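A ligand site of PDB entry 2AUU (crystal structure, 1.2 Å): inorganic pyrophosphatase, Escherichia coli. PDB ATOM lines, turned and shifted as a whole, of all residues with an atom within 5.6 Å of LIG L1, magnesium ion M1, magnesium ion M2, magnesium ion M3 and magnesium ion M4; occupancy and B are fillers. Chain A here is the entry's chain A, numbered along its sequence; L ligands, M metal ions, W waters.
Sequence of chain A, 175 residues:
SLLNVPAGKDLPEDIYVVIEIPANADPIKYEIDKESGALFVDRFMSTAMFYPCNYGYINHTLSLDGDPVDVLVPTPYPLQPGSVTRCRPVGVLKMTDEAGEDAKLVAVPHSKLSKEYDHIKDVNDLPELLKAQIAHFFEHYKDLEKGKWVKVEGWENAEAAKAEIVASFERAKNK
NZ of Lys 104 lies close to O5 of LIG L1, 3.8 Å away.
NH2 of Arg 43 is in salt-bridge range of O2 of LIG L1, at 2.8 Å.
The side-chain hydroxyl (OH) of Tyr 55 sits close to an oxygen (O6) of LIG L1 (2.7 Å).
An oxygen (O2) of LIG L1 is in salt-bridge range of the side-chain amino group (NZ) of Lys 142 (3.8 Å).
The side-chain hydroxyl (OH) of Tyr 141 sits at hydrogen-bond distance from an oxygen (O2) of LIG L1 (2.8 Å).
The side-chain amino group (NZ) of Lys 29 sits at hydrogen-bond distance from an oxygen (O4) of LIG L1, at 2.9 Å.
The side-chain amino group of Lys 29 sits close to the side-chain carboxylate of Glu 31, 2.8 Å away.
The backbone NH (N) of Asp 67 sits at hydrogen-bond distance from the side-chain carboxylate (OD2) of Asp 65 (3.1 Å).
The side-chain amino group (NZ) of Lys 142 sits close to the side-chain hydroxyl (OH) of Tyr 141 (3.5 Å).
The side-chain carboxylate (OD2) of Asp 70 lies close to the side-chain hydroxyl (OH) of Tyr 55 (3.2 Å).
O of Asp 102 sits at hydrogen-bond distance from NZ of Lys 104 (3.1 Å).
The backbone NH (N) of Asp 42 is in hydrogen-bond range of the backbone carbonyl oxygen (O) of Lys 29.
The side-chain amino group (NZ) of Lys 142 sits close to the side-chain carboxylate (OD2) of Asp 97 (2.6 Å).
N of Lys 29 sits at hydrogen-bond distance from O of Arg 43.
The side-chain carboxylate of Asp 67 lies close to an oxygen (O7) of LIG L1, 3.0 Å away.
OD2 of Asp 67 touches magnesium ion M1, at 3.9 Å.
Lys 104 touches magnesium ion M1.
Within 4 Å of magnesium ion M1: Asp 65, Asp 67, Asp 70, Asp 102 and Lys 104.
Along chain A the residues within 4 Å of magnesium ion M1 span positions 65 to 104.
Tyr 55 touches magnesium ion M2 (OH to MG, 3.9 Å).
Asp 67 touches magnesium ion M2.
Three residues have an atom within 4 Å of magnesium ion M2: Tyr 55, Asp 67 and Asp 70.
The nearest printed residue that does not touch magnesium ion M2 is Pro 68 (4.1 Å).
Merely in contact with magnesium ion M3: Lys 142 (3.7 Å) and Lys 104 (3.98 Å).
Of the 22 residues printed, 5 come within 4 Å of magnesium ion M3.
The nearest printed residue that does not touch magnesium ion M3 is Tyr 141 (4.1 Å).
NZ of Lys 29 touches magnesium ion M4, 3.9 Å away.
OD2 of Asp 67 touches magnesium ion M4, 3.8 Å away.
The side-chain carboxylate (OD1) of Asp 65 binds magnesium ion M1 (1.9 Å).
Magnesium ion M1 is bound by O5 of LIG L1 (2.0 Å).
A fluorine (F1) of LG2 L2 binds magnesium ion M1 (2.0 Å).
The side-chain carboxylate (OD1) of Asp 102 binds magnesium ion M1, at 2.1 Å.
The side-chain carboxylate (OD2) of Asp 70 is bound to magnesium ion M1 (2.1 Å).
Water W5 binds magnesium ion M1, at 2.2 Å.
Magnesium ion M1 has six donor atoms within binding distance.
Magnesium ion M2 is bound by a fluorine (F1) of LG2 L2 (1.9 Å), water W3 (2.1 Å), an oxygen (O6) of LIG L1 (2.1 Å), water W9 (2.1 Å), the side-chain carboxylate (OD1) of Asp 70 (2.1 Å) and water W4 (2.1 Å).
Magnesium ion M3 is bound by the side-chain carboxylate (OD2) of Asp 97 (2.0 Å), an oxygen (O1) of LIG L1 (2.0 Å), water W10 (2.1 Å), the side-chain carboxylate (OD2) of Asp 102 (2.1 Å), water W2 (2.1 Å) and an oxygen (O5) of LIG L1 (2.2 Å).
Magnesium ion M4 is bound by O3 of LIG L1 (2.0 Å), O7 of LIG L1 (2.0 Å), water W6 (2.0 Å), water W1 (2.0 Å), water W8 (2.0 Å) and OE2 of Glu 31 (2.1 Å).
Water W5 bridges the side-chain carboxylate (OD2) of Asp 65 (2.7 Å) and the backbone carbonyl oxygen (O) of Pro 68 (2.9 Å).
Water W2 lies within hydrogen-bond range of OH of Tyr 141 (2.7 Å), NZ of Lys 104 (3.0 Å) and O4 of LIG L1 (3.5 Å).
Water W1 bridges the side-chain carboxylate (OE1) of Glu 31 (2.7 Å) and the side-chain carboxylate (OD2) of Asp 67 (2.7 Å).
Water W6 lies within hydrogen-bond range of OD2 of Asp 42 and NH1 of Arg 43.
Water W7 lies within hydrogen-bond range of the side-chain hydroxyl (OH) of Tyr 51 (2.7 Å), an oxygen (O4) of LIG L1 (3.0 Å), the side-chain hydroxyl (OH) of Tyr 55 (3.2 Å) and the side-chain hydroxyl (OH) of Tyr 141 (3.3 Å).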
ATOM      1  N   GLU A  20      12.292  -9.986 -25.690  1.00  0.00           N
ATOM      2  CA  GLU A  20      13.270  -9.677 -24.647  1.00  0.00           C
ATOM      3  C   GLU A  20      14.224 -10.814 -24.314  1.00  0.00           C
ATOM      4  O   GLU A  20      15.368 -10.581 -24.019  1.00  0.00           O
ATOM      5  CB  GLU A  20      12.510  -9.275 -23.388  1.00  0.00           C
ATOM      6  CG  GLU A  20      11.802  -7.928 -23.592  1.00  0.00           C
ATOM      7  CD  GLU A  20      10.832  -7.656 -22.432  1.00  0.00           C
ATOM      8  OE1 GLU A  20      10.110  -8.579 -22.068  1.00  0.00           O
ATOM      9  OE2 GLU A  20      10.852  -6.481 -21.928  1.00  0.00           O
ATOM     10  N   LYS A  29      17.410 -12.449 -17.278  1.00  0.00           N
ATOM     11  CA  LYS A  29      16.059 -11.921 -17.494  1.00  0.00           C
ATOM     12  C   LYS A  29      16.165 -10.488 -17.939  1.00  0.00           C
ATOM     13  O   LYS A  29      16.294  -9.588 -17.147  1.00  0.00           O
ATOM     14  CB  LYS A  29      15.264 -12.078 -16.217  1.00  0.00           C
ATOM     15  CG  LYS A  29      13.826 -12.117 -16.378  1.00  0.00           C
ATOM     16  CD  LYS A  29      13.077 -11.001 -16.953  1.00  0.00           C
ATOM     17  CE  LYS A  29      11.577 -11.391 -17.018  1.00  0.00           C
ATOM     18  NZ  LYS A  29      10.726 -10.267 -17.524  1.00  0.00           N
ATOM     19  N   GLU A  31      14.673  -6.990 -19.680  1.00  0.00           N
ATOM     20  CA  GLU A  31      13.442  -6.273 -19.866  1.00  0.00           C
ATOM     21  C   GLU A  31      13.742  -4.964 -20.566  1.00  0.00           C
ATOM     22  O   GLU A  31      14.669  -4.281 -20.159  1.00  0.00           O
ATOM     23  CB  GLU A  31      12.721  -6.002 -18.533  1.00  0.00           C
ATOM     24  CG  GLU A  31      12.237  -7.265 -17.832  1.00  0.00           C
ATOM     25  CD  GLU A  31      11.381  -6.998 -16.608  1.00  0.00           C
ATOM     26  OE1 GLU A  31      11.172  -5.842 -16.205  1.00  0.00           O
ATOM     27  OE2 GLU A  31      10.862  -7.977 -15.965  1.00  0.00           O
ATOM     28  N   ASP A  42      17.164  -7.256 -15.883  1.00  0.00           N
ATOM     29  CA  ASP A  42      16.318  -7.119 -14.735  1.00  0.00           C
ATOM     30  C   ASP A  42      16.899  -7.924 -13.596  1.00  0.00           C
ATOM     31  O   ASP A  42      16.989  -7.447 -12.450  1.00  0.00           O
ATOM     32  CB  ASP A  42      14.859  -7.498 -15.065  1.00  0.00           C
ATOM     33  CG  ASP A  42      13.984  -7.261 -13.862  1.00  0.00           C
ATOM     34  OD1 ASP A  42      13.719  -6.108 -13.495  1.00  0.00           O
ATOM     35  OD2 ASP A  42      13.586  -8.227 -13.244  1.00  0.00           O
ATOM     36  N   ARG A  43      17.270  -9.171 -13.882  1.00  0.00           N
ATOM     37  CA  ARG A  43      17.958  -9.986 -12.898  1.00  0.00           C
ATOM     38  C   ARG A  43      18.584 -11.202 -13.586  1.00  0.00           C
ATOM     39  O   ARG A  43      18.321 -11.479 -14.759  1.00  0.00           O
ATOM     40  CB  ARG A  43      17.008 -10.410 -11.838  1.00  0.00           C
ATOM     41  CG  ARG A  43      15.968 -11.390 -12.374  1.00  0.00           C
ATOM     42  CD  ARG A  43      14.795 -11.434 -11.431  1.00  0.00           C
ATOM     43  NE  ARG A  43      13.763 -12.382 -11.838  1.00  0.00           N
ATOM     44  CZ  ARG A  43      12.686 -12.111 -12.582  1.00  0.00           C
ATOM     45  NH1 ARG A  43      12.428 -10.876 -13.062  1.00  0.00           N
ATOM     46  NH2 ARG A  43      11.814 -13.109 -12.868  1.00  0.00           N
ATOM     47  N   TYR A  51      13.352 -20.254 -20.606  1.00  0.00           N
ATOM     48  CA  TYR A  51      12.047 -19.997 -21.179  1.00  0.00           C
ATOM     49  C   TYR A  51      11.771 -20.996 -22.314  1.00  0.00           C
ATOM     50  O   TYR A  51      12.628 -21.126 -23.225  1.00  0.00           O
ATOM     51  CB  TYR A  51      11.899 -18.595 -21.748  1.00  0.00           C
ATOM     52  CG  TYR A  51      11.715 -17.572 -20.658  1.00  0.00           C
ATOM     53  CD1 TYR A  51      12.734 -17.089 -19.865  1.00  0.00           C
ATOM     54  CD2 TYR A  51      10.448 -17.025 -20.375  1.00  0.00           C
ATOM     55  CE1 TYR A  51      12.593 -16.173 -18.863  1.00  0.00           C
ATOM     56  CE2 TYR A  51      10.282 -16.107 -19.377  1.00  0.00           C
ATOM     57  CZ  TYR A  51      11.345 -15.674 -18.609  1.00  0.00           C
ATOM     58  OH  TYR A  51      11.220 -14.764 -17.632  1.00  0.00           O
ATOM     59  N   TYR A  55      10.334 -14.882 -25.417  1.00  0.00           N
ATOM     60  CA  TYR A  55       9.489 -14.177 -24.479  1.00  0.00           C
ATOM     61  C   TYR A  55       9.628 -12.663 -24.674  1.00  0.00           C
ATOM     62  O   TYR A  55      10.733 -12.158 -24.791  1.00  0.00           O
ATOM     63  CB  TYR A  55       9.902 -14.526 -23.075  1.00  0.00           C
ATOM     64  CG  TYR A  55       9.102 -13.891 -21.980  1.00  0.00           C
ATOM     65  CD1 TYR A  55       7.865 -14.414 -21.644  1.00  0.00           C
ATOM     66  CD2 TYR A  55       9.559 -12.803 -21.268  1.00  0.00           C
ATOM     67  CE1 TYR A  55       7.127 -13.857 -20.648  1.00  0.00           C
ATOM     68  CE2 TYR A  55       8.814 -12.228 -20.273  1.00  0.00           C
ATOM     69  CZ  TYR A  55       7.593 -12.757 -19.961  1.00  0.00           C
ATOM     70  OH  TYR A  55       6.772 -12.275 -18.961  1.00  0.00           O
ATOM     71  N   GLY A  56       8.487 -11.957 -24.704  1.00  0.00           N
ATOM     72  CA  GLY A  56       8.526 -10.521 -24.816  1.00  0.00           C
ATOM     73  C   GLY A  56       7.182  -9.916 -24.500  1.00  0.00           C
ATOM     74  O   GLY A  56       6.473 -10.375 -23.628  1.00  0.00           O
ATOM     75  N   TYR A  57       6.850  -8.874 -25.243  1.00  0.00           N
ATOM     76  CA  TYR A  57       5.626  -8.086 -24.969  1.00  0.00           C
ATOM     77  C   TYR A  57       5.071  -7.449 -26.213  1.00  0.00           C
ATOM     78  O   TYR A  57       5.718  -7.355 -27.239  1.00  0.00           O
ATOM     79  CB  TYR A  57       5.972  -7.040 -23.872  1.00  0.00           C
ATOM     80  CG  TYR A  57       6.905  -5.999 -24.346  1.00  0.00           C
ATOM     81  CD1 TYR A  57       8.255  -6.203 -24.278  1.00  0.00           C
ATOM     82  CD2 TYR A  57       6.505  -4.779 -24.900  1.00  0.00           C
ATOM     83  CE1 TYR A  57       9.122  -5.229 -24.723  1.00  0.00           C
ATOM     84  CE2 TYR A  57       7.380  -3.781 -25.361  1.00  0.00           C
ATOM     85  CZ  TYR A  57       8.716  -4.054 -25.277  1.00  0.00           C
ATOM     86  OH  TYR A  57       9.655  -3.146 -25.679  1.00  0.00           O
ATOM     87  N   SER A  63      -0.575  -4.196 -18.811  1.00  0.00           N
ATOM     88  CA  SER A  63      -1.099  -5.206 -17.920  1.00  0.00           C
ATOM     89  C   SER A  63      -1.264  -4.682 -16.489  1.00  0.00           C
ATOM     90  O   SER A  63      -0.973  -3.530 -16.330  1.00  0.00           O
ATOM     91  CB  SER A  63      -0.174  -6.467 -17.874  1.00  0.00           C
ATOM     92  OG  SER A  63      -0.541  -7.107 -19.053  1.00  0.00           O
ATOM     93  N   ASP A  65       0.455  -5.670 -13.871  1.00  0.00           N
ATOM     94  CA  ASP A  65       1.736  -5.781 -13.211  1.00  0.00           C
ATOM     95  C   ASP A  65       2.609  -4.538 -13.512  1.00  0.00           C
ATOM     96  O   ASP A  65       3.787  -4.501 -13.131  1.00  0.00           O
ATOM     97  CB  ASP A  65       2.483  -7.082 -13.603  1.00  0.00           C
ATOM     98  CG  ASP A  65       3.067  -7.131 -14.998  1.00  0.00           C
ATOM     99  OD1 ASP A  65       3.994  -7.938 -15.279  1.00  0.00           O
ATOM    100  OD2 ASP A  65       2.528  -6.322 -15.780  1.00  0.00           O
ATOM    101  N   ASP A  67       3.398  -3.472 -16.494  1.00  0.00           N
ATOM    102  CA  ASP A  67       4.259  -3.709 -17.609  1.00  0.00           C
ATOM    103  C   ASP A  67       3.365  -3.932 -18.837  1.00  0.00           C
ATOM    104  O   ASP A  67       2.260  -4.301 -18.573  1.00  0.00           O
ATOM    105  CB  ASP A  67       5.120  -4.953 -17.401  1.00  0.00           C
ATOM    106  CG  ASP A  67       6.149  -4.987 -16.315  1.00  0.00           C
ATOM    107  OD1 ASP A  67       6.374  -3.890 -15.750  1.00  0.00           O
ATOM    108  OD2 ASP A  67       6.771  -6.037 -15.978  1.00  0.00           O
ATOM    109  N   PRO A  68       3.798  -3.795 -20.084  1.00  0.00           N
ATOM    110  CA  PRO A  68       3.068  -4.328 -21.264  1.00  0.00           C
ATOM    111  C   PRO A  68       2.743  -5.812 -21.190  1.00  0.00           C
ATOM    112  O   PRO A  68       3.472  -6.565 -20.512  1.00  0.00           O
ATOM    113  CB  PRO A  68       4.082  -4.130 -22.378  1.00  0.00           C
ATOM    114  CG  PRO A  68       4.916  -2.935 -21.956  1.00  0.00           C
ATOM    115  CD  PRO A  68       5.055  -3.086 -20.488  1.00  0.00           C
ATOM    116  N   ASP A  70       2.516  -9.624 -21.726  1.00  0.00           N
ATOM    117  CA  ASP A  70       3.585 -10.579 -21.981  1.00  0.00           C
ATOM    118  C   ASP A  70       3.166 -11.664 -22.904  1.00  0.00           C
ATOM    119  O   ASP A  70       2.016 -12.181 -22.867  1.00  0.00           O
ATOM    120  CB  ASP A  70       3.971 -11.189 -20.642  1.00  0.00           C
ATOM    121  CG  ASP A  70       4.555 -10.238 -19.606  1.00  0.00           C
ATOM    122  OD1 ASP A  70       5.361  -9.394 -20.044  1.00  0.00           O
ATOM    123  OD2 ASP A  70       4.301 -10.405 -18.394  1.00  0.00           O
ATOM    124  N   MET A  95      -2.315 -16.242 -15.008  1.00  0.00           N
ATOM    125  CA  MET A  95      -1.544 -16.291 -13.775  1.00  0.00           C
ATOM    126  C   MET A  95      -1.385 -14.883 -13.137  1.00  0.00           C
ATOM    127  O   MET A  95      -1.491 -13.849 -13.847  1.00  0.00           O
ATOM    128  CB  MET A  95      -0.173 -16.934 -13.987  1.00  0.00           C
ATOM    129  CG  MET A  95       0.513 -16.331 -15.202  1.00  0.00           C
ATOM    130  SD  MET A  95       2.305 -16.281 -14.973  1.00  0.00           S
ATOM    131  CE  MET A  95       2.407 -15.049 -13.671  1.00  0.00           C
ATOM    132  N   ASP A  97       1.354 -12.547 -10.345  1.00  0.00           N
ATOM    133  CA  ASP A  97       2.642 -12.705  -9.616  1.00  0.00           C
ATOM    134  C   ASP A  97       2.697 -11.532  -8.648  1.00  0.00           C
ATOM    135  O   ASP A  97       1.704 -10.821  -8.468  1.00  0.00           O
ATOM    136  CB  ASP A  97       3.840 -12.884 -10.497  1.00  0.00           C
ATOM    137  CG  ASP A  97       4.399 -11.740 -11.336  1.00  0.00           C
ATOM    138  OD1 ASP A  97       3.921 -10.619 -11.042  1.00  0.00           O
ATOM    139  OD2 ASP A  97       5.231 -11.911 -12.233  1.00  0.00           O
ATOM    140  N   GLU A  98       3.879 -11.393  -8.011  1.00  0.00           N
ATOM    141  CA  GLU A  98       4.012 -10.390  -6.964  1.00  0.00           C
ATOM    142  C   GLU A  98       3.694  -8.983  -7.434  1.00  0.00           C
ATOM    143  O   GLU A  98       3.332  -8.183  -6.583  1.00  0.00           O
ATOM    144  CB  GLU A  98       5.432 -10.443  -6.425  1.00  0.00           C
ATOM    145  CG  GLU A  98       6.505  -9.733  -7.241  1.00  0.00           C
ATOM    146  CD  GLU A  98       7.004 -10.576  -8.428  1.00  0.00           C
ATOM    147  OE1 GLU A  98       6.814 -11.849  -8.385  1.00  0.00           O
ATOM    148  OE2 GLU A  98       7.541  -9.863  -9.336  1.00  0.00           O
ATOM    149  N   ASP A 102      -0.949 -11.016 -14.330  1.00  0.00           N
ATOM    150  CA  ASP A 102       0.126 -11.077 -15.313  1.00  0.00           C
ATOM    151  C   ASP A 102      -0.010 -12.196 -16.298  1.00  0.00           C
ATOM    152  O   ASP A 102       0.888 -13.043 -16.345  1.00  0.00           O
ATOM    153  CB  ASP A 102       1.393 -11.202 -14.446  1.00  0.00           C
ATOM    154  CG  ASP A 102       2.626 -10.802 -15.192  1.00  0.00           C
ATOM    155  OD1 ASP A 102       2.679 -10.103 -16.258  1.00  0.00           O
ATOM    156  OD2 ASP A 102       3.669 -11.277 -14.605  1.00  0.00           O
ATOM    157  N   LYS A 104       0.065 -14.702 -19.478  1.00  0.00           N
ATOM    158  CA  LYS A 104       1.102 -15.087 -20.428  1.00  0.00           C
ATOM    159  C   LYS A 104       0.417 -15.589 -21.742  1.00  0.00           C
ATOM    160  O   LYS A 104      -0.073 -16.685 -21.834  1.00  0.00           O
ATOM    161  CB  LYS A 104       2.030 -16.126 -19.905  1.00  0.00           C
ATOM    162  CG  LYS A 104       2.733 -15.714 -18.603  1.00  0.00           C
ATOM    163  CD  LYS A 104       3.780 -14.669 -18.836  1.00  0.00           C
ATOM    164  CE  LYS A 104       4.411 -14.199 -17.523  1.00  0.00           C
ATOM    165  NZ  LYS A 104       3.855 -12.928 -17.095  1.00  0.00           N
ATOM    166  N   TYR A 141       9.831 -20.964 -11.815  1.00  0.00           N
ATOM    167  CA  TYR A 141      11.009 -20.150 -12.109  1.00  0.00           C
ATOM    168  C   TYR A 141      11.332 -19.124 -11.002  1.00  0.00           C
ATOM    169  O   TYR A 141      12.482 -18.708 -10.950  1.00  0.00           O
ATOM    170  CB  TYR A 141      10.899 -19.476 -13.451  1.00  0.00           C
ATOM    171  CG  TYR A 141      10.038 -18.237 -13.564  1.00  0.00           C
ATOM    172  CD1 TYR A 141       8.686 -18.206 -13.099  1.00  0.00           C
ATOM    173  CD2 TYR A 141      10.580 -17.084 -14.147  1.00  0.00           C
ATOM    174  CE1 TYR A 141       7.953 -17.016 -13.249  1.00  0.00           C
ATOM    175  CE2 TYR A 141       9.858 -15.932 -14.274  1.00  0.00           C
ATOM    176  CZ  TYR A 141       8.549 -15.906 -13.819  1.00  0.00           C
ATOM    177  OH  TYR A 141       7.750 -14.740 -13.927  1.00  0.00           O
ATOM    178  N   LYS A 142      10.396 -18.760 -10.171  1.00  0.00           N
ATOM    179  CA  LYS A 142      10.602 -17.834  -9.089  1.00  0.00           C
ATOM    180  C   LYS A 142      10.799 -18.507  -7.750  1.00  0.00           C
ATOM    181  O   LYS A 142      10.746 -17.792  -6.740  1.00  0.00           O
ATOM    182  CB  LYS A 142       9.402 -16.846  -9.055  1.00  0.00           C
ATOM    183  CG  LYS A 142       9.550 -15.760 -10.181  1.00  0.00           C
ATOM    184  CD  LYS A 142       8.344 -14.837 -10.302  1.00  0.00           C
ATOM    185  CE  LYS A 142       8.692 -13.481 -10.908  1.00  0.00           C
ATOM    186  NZ  LYS A 142       7.518 -12.662 -11.179  1.00  0.00           N
ATOM    187  N   LYS A 148       9.282 -12.860  -4.868  1.00  0.00           N
ATOM    188  CA  LYS A 148       8.746 -13.038  -6.213  1.00  0.00           C
ATOM    189  C   LYS A 148       7.878 -14.294  -6.174  1.00  0.00           C
ATOM    190  O   LYS A 148       8.319 -15.294  -5.626  1.00  0.00           O
ATOM    191  CB  LYS A 148       9.744 -13.263  -7.305  1.00  0.00           C
ATOM    192  CG  LYS A 148      10.820 -12.171  -7.302  1.00  0.00           C
ATOM    193  CD  LYS A 148      10.552 -10.910  -8.014  1.00  0.00           C
ATOM    194  CE  LYS A 148      11.761 -10.258  -8.721  1.00  0.00           C
ATOM    195  NZ  LYS A 148      11.307  -8.990  -9.383  1.00  0.00           N
HETATM  196  P1  LIG L   1       8.815 -11.307 -14.392  1.00  0.00           P
HETATM  197  O1  LIG L   1       7.631 -11.168 -13.549  1.00  0.00           O
HETATM  198  O2  LIG L   1       9.481 -12.640 -14.430  1.00  0.00           O
HETATM  199  O3  LIG L   1       9.799 -10.137 -14.281  1.00  0.00           O
HETATM  200  O4  LIG L   1       8.339 -11.112 -16.016  1.00  0.00           O
HETATM  201  P2  LIG L   1       7.424  -9.847 -16.423  1.00  0.00           P
HETATM  202  O5  LIG L   1       6.014 -10.051 -15.923  1.00  0.00           O
HETATM  203  O6  LIG L   1       7.549  -9.906 -17.898  1.00  0.00           O
HETATM  204  O7  LIG L   1       8.132  -8.686 -15.750  1.00  0.00           O
HETATM  205  F1  LG2 L   2       5.825  -7.870 -17.587  1.00  0.00           F
HETATM  206 MG    MG M   1       4.452  -9.102 -16.738  1.00  0.00          MG
HETATM  207 MG    MG M   2       6.900  -8.358 -19.098  1.00  0.00          MG
HETATM  208 MG    MG M   3       5.680 -11.165 -14.027  1.00  0.00          MG
HETATM  209 MG    MG M   4       9.501  -8.207 -14.392  1.00  0.00          MG
HETATM  210  O   HOH W   1       9.071  -6.247 -14.565  1.00  0.00           O
HETATM  211  O   HOH W   2       5.777 -13.149 -14.829  1.00  0.00           O
HETATM  212  O   HOH W   3       6.266  -6.651 -20.045  1.00  0.00           O
HETATM  213  O   HOH W   4       8.561  -7.336 -18.269  1.00  0.00           O
HETATM  214  O   HOH W   5       3.027  -7.875 -17.932  1.00  0.00           O
HETATM  215  O   HOH W   6      10.859  -7.762 -12.972  1.00  0.00           O
HETATM  216  O   HOH W   7       8.689 -13.881 -17.021  1.00  0.00           O
HETATM  217  O   HOH W   8       8.069  -8.204 -12.943  1.00  0.00           O
HETATM  218  O   HOH W   9       7.965  -8.946 -20.779  1.00  0.00           O
HETATM  219  O   HOH W  10       5.312  -9.326 -13.188  1.00  0.00           O
